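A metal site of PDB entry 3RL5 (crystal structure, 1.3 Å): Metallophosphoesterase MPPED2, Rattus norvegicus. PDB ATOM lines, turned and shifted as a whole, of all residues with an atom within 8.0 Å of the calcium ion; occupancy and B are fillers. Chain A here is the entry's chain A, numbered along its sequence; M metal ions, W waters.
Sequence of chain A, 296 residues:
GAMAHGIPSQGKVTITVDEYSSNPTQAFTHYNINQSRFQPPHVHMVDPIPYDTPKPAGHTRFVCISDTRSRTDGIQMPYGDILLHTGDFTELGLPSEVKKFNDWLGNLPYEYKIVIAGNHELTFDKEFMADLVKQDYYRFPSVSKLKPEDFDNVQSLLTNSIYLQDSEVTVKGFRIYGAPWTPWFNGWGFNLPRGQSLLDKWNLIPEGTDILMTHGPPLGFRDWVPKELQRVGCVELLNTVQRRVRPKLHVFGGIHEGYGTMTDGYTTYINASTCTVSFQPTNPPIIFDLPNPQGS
The nearest printed residue that does not touch the calcium ion is Asp 150 (4.5 Å).
The calcium ion is bound by the backbone carbonyl oxygen of Glu 149 (2.3 Å), the side-chain carboxylate of Asp 152 (2.4 Å), water W1 (2.4 Å), the side-chain carboxylate of Glu 149 (2.4 Å) and the side-chain amide oxygen of Asn 153 (2.6 Å). The calcium ion has five donor atoms within binding distance.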
ATOM      1  N   PRO A  95      22.197 -13.766  -7.380  1.00  0.00           N
ATOM      2  CA  PRO A  95      22.492 -15.153  -7.709  1.00  0.00           C
ATOM      3  C   PRO A  95      23.815 -15.695  -7.126  1.00  0.00           C
ATOM      4  O   PRO A  95      23.866 -16.831  -6.639  1.00  0.00           O
ATOM      5  CB  PRO A  95      22.462 -15.158  -9.251  1.00  0.00           C
ATOM      6  CG  PRO A  95      21.461 -14.069  -9.557  1.00  0.00           C
ATOM      7  CD  PRO A  95      21.706 -13.009  -8.554  1.00  0.00           C
ATOM      8  N   LYS A 147      19.518  -8.793 -15.353  1.00  0.00           N
ATOM      9  CA  LYS A 147      18.647  -9.068 -16.481  1.00  0.00           C
ATOM     10  C   LYS A 147      17.678 -10.185 -16.083  1.00  0.00           C
ATOM     11  O   LYS A 147      18.016 -11.001 -15.201  1.00  0.00           O
ATOM     12  CB  LYS A 147      19.449  -9.494 -17.710  1.00  0.00           C
ATOM     13  CG  LYS A 147      20.520  -8.498 -18.143  1.00  0.00           C
ATOM     14  CD  LYS A 147      19.934  -7.477 -19.088  1.00  0.00           C
ATOM     15  CE  LYS A 147      21.005  -6.481 -19.521  1.00  0.00           C
ATOM     16  NZ  LYS A 147      20.483  -5.471 -20.467  1.00  0.00           N
ATOM     17  N   PRO A 148      16.492 -10.240 -16.705  1.00  0.00           N
ATOM     18  CA  PRO A 148      15.546 -11.311 -16.388  1.00  0.00           C
ATOM     19  C   PRO A 148      16.195 -12.694 -16.363  1.00  0.00           C
ATOM     20  O   PRO A 148      15.882 -13.494 -15.473  1.00  0.00           O
ATOM     21  CB  PRO A 148      14.506 -11.204 -17.494  1.00  0.00           C
ATOM     22  CG  PRO A 148      14.470  -9.724 -17.769  1.00  0.00           C
ATOM     23  CD  PRO A 148      15.924  -9.320 -17.722  1.00  0.00           C
ATOM     24  N   GLU A 149      17.105 -12.970 -17.299  1.00  0.00           N
ATOM     25  CA  GLU A 149      17.774 -14.272 -17.362  1.00  0.00           C
ATOM     26  C   GLU A 149      18.704 -14.557 -16.178  1.00  0.00           C
ATOM     27  O   GLU A 149      19.035 -15.713 -15.907  1.00  0.00           O
ATOM     28  CB  GLU A 149      18.527 -14.439 -18.694  1.00  0.00           C
ATOM     29  CG  GLU A 149      19.144 -15.834 -18.922  1.00  0.00           C
ATOM     30  CD  GLU A 149      18.106 -16.969 -18.970  1.00  0.00           C
ATOM     31  OE1 GLU A 149      17.091 -16.795 -19.688  1.00  0.00           O
ATOM     32  OE2 GLU A 149      18.293 -18.046 -18.276  1.00  0.00           O
ATOM     33  N   ASP A 150      19.127 -13.506 -15.478  1.00  0.00           N
ATOM     34  CA  ASP A 150      20.010 -13.680 -14.325  1.00  0.00           C
ATOM     35  C   ASP A 150      19.283 -14.215 -13.091  1.00  0.00           C
ATOM     36  O   ASP A 150      19.918 -14.822 -12.222  1.00  0.00           O
ATOM     37  CB  ASP A 150      20.701 -12.369 -13.944  1.00  0.00           C
ATOM     38  CG  ASP A 150      21.594 -11.812 -15.032  1.00  0.00           C
ATOM     39  OD1 ASP A 150      22.194 -12.602 -15.804  1.00  0.00           O
ATOM     40  OD2 ASP A 150      21.712 -10.575 -15.125  1.00  0.00           O
ATOM     41  N   PHE A 151      17.982 -14.004 -12.989  1.00  0.00           N
ATOM     42  CA  PHE A 151      17.270 -14.407 -11.781  1.00  0.00           C
ATOM     43  C   PHE A 151      16.013 -15.226 -12.025  1.00  0.00           C
ATOM     44  O   PHE A 151      15.261 -15.501 -11.078  1.00  0.00           O
ATOM     45  CB  PHE A 151      17.003 -13.188 -10.879  1.00  0.00           C
ATOM     46  CG  PHE A 151      16.092 -12.170 -11.485  1.00  0.00           C
ATOM     47  CD1 PHE A 151      14.718 -12.218 -11.273  1.00  0.00           C
ATOM     48  CD2 PHE A 151      16.608 -11.126 -12.276  1.00  0.00           C
ATOM     49  CE1 PHE A 151      13.876 -11.277 -11.836  1.00  0.00           C
ATOM     50  CE2 PHE A 151      15.761 -10.177 -12.836  1.00  0.00           C
ATOM     51  CZ  PHE A 151      14.397 -10.255 -12.625  1.00  0.00           C
ATOM     52  N   ASP A 152      15.801 -15.673 -13.265  1.00  0.00           N
ATOM     53  CA  ASP A 152      14.648 -16.518 -13.548  1.00  0.00           C
ATOM     54  C   ASP A 152      14.777 -17.893 -12.878  1.00  0.00           C
ATOM     55  O   ASP A 152      13.767 -18.508 -12.550  1.00  0.00           O
ATOM     56  CB  ASP A 152      14.343 -16.626 -15.073  1.00  0.00           C
ATOM     57  CG  ASP A 152      15.450 -17.320 -15.874  1.00  0.00           C
ATOM     58  OD1 ASP A 152      16.631 -17.324 -15.445  1.00  0.00           O
ATOM     59  OD2 ASP A 152      15.156 -17.837 -16.982  1.00  0.00           O
ATOM     60  N   ASN A 153      16.005 -18.351 -12.645  1.00  0.00           N
ATOM     61  CA  ASN A 153      16.270 -19.663 -12.057  1.00  0.00           C
ATOM     62  C   ASN A 153      16.907 -19.579 -10.666  1.00  0.00           C
ATOM     63  O   ASN A 153      17.611 -20.490 -10.249  1.00  0.00           O
ATOM     64  CB  ASN A 153      17.133 -20.498 -12.990  1.00  0.00           C
ATOM     65  CG  ASN A 153      18.525 -19.912 -13.184  1.00  0.00           C
ATOM     66  OD1 ASN A 153      18.709 -18.690 -13.396  1.00  0.00           O
ATOM     67  ND2 ASN A 153      19.524 -20.794 -13.184  1.00  0.00           N
ATOM     68  N   VAL A 154      16.663 -18.471  -9.970  1.00  0.00           N
ATOM     69  CA  VAL A 154      17.288 -18.279  -8.702  1.00  0.00           C
ATOM     70  C   VAL A 154      16.972 -19.376  -7.675  1.00  0.00           C
ATOM     71  O   VAL A 154      17.891 -19.924  -7.137  1.00  0.00           O
ATOM     72  CB  VAL A 154      17.189 -16.825  -8.200  1.00  0.00           C
ATOM     73  CG1 VAL A 154      15.867 -16.524  -7.497  1.00  0.00           C
ATOM     74  CG2 VAL A 154      18.413 -16.480  -7.386  1.00  0.00           C
ATOM     75  N   LEU A 157      18.933 -22.646  -7.913  1.00  0.00           N
ATOM     76  CA  LEU A 157      20.328 -22.671  -7.474  1.00  0.00           C
ATOM     77  C   LEU A 157      20.488 -23.378  -6.131  1.00  0.00           C
ATOM     78  O   LEU A 157      21.598 -23.771  -5.771  1.00  0.00           O
ATOM     79  CB  LEU A 157      20.898 -21.257  -7.393  1.00  0.00           C
ATOM     80  CG  LEU A 157      20.982 -20.507  -8.732  1.00  0.00           C
ATOM     81  CD1 LEU A 157      21.448 -19.070  -8.468  1.00  0.00           C
ATOM     82  CD2 LEU A 157      21.928 -21.244  -9.720  1.00  0.00           C
HETATM   83 CA    CA M   1      18.852 -17.977 -15.909  1.00  0.00          CA
HETATM   84  O   HOH W   1      21.124 -17.829 -15.124  1.00  0.00           O
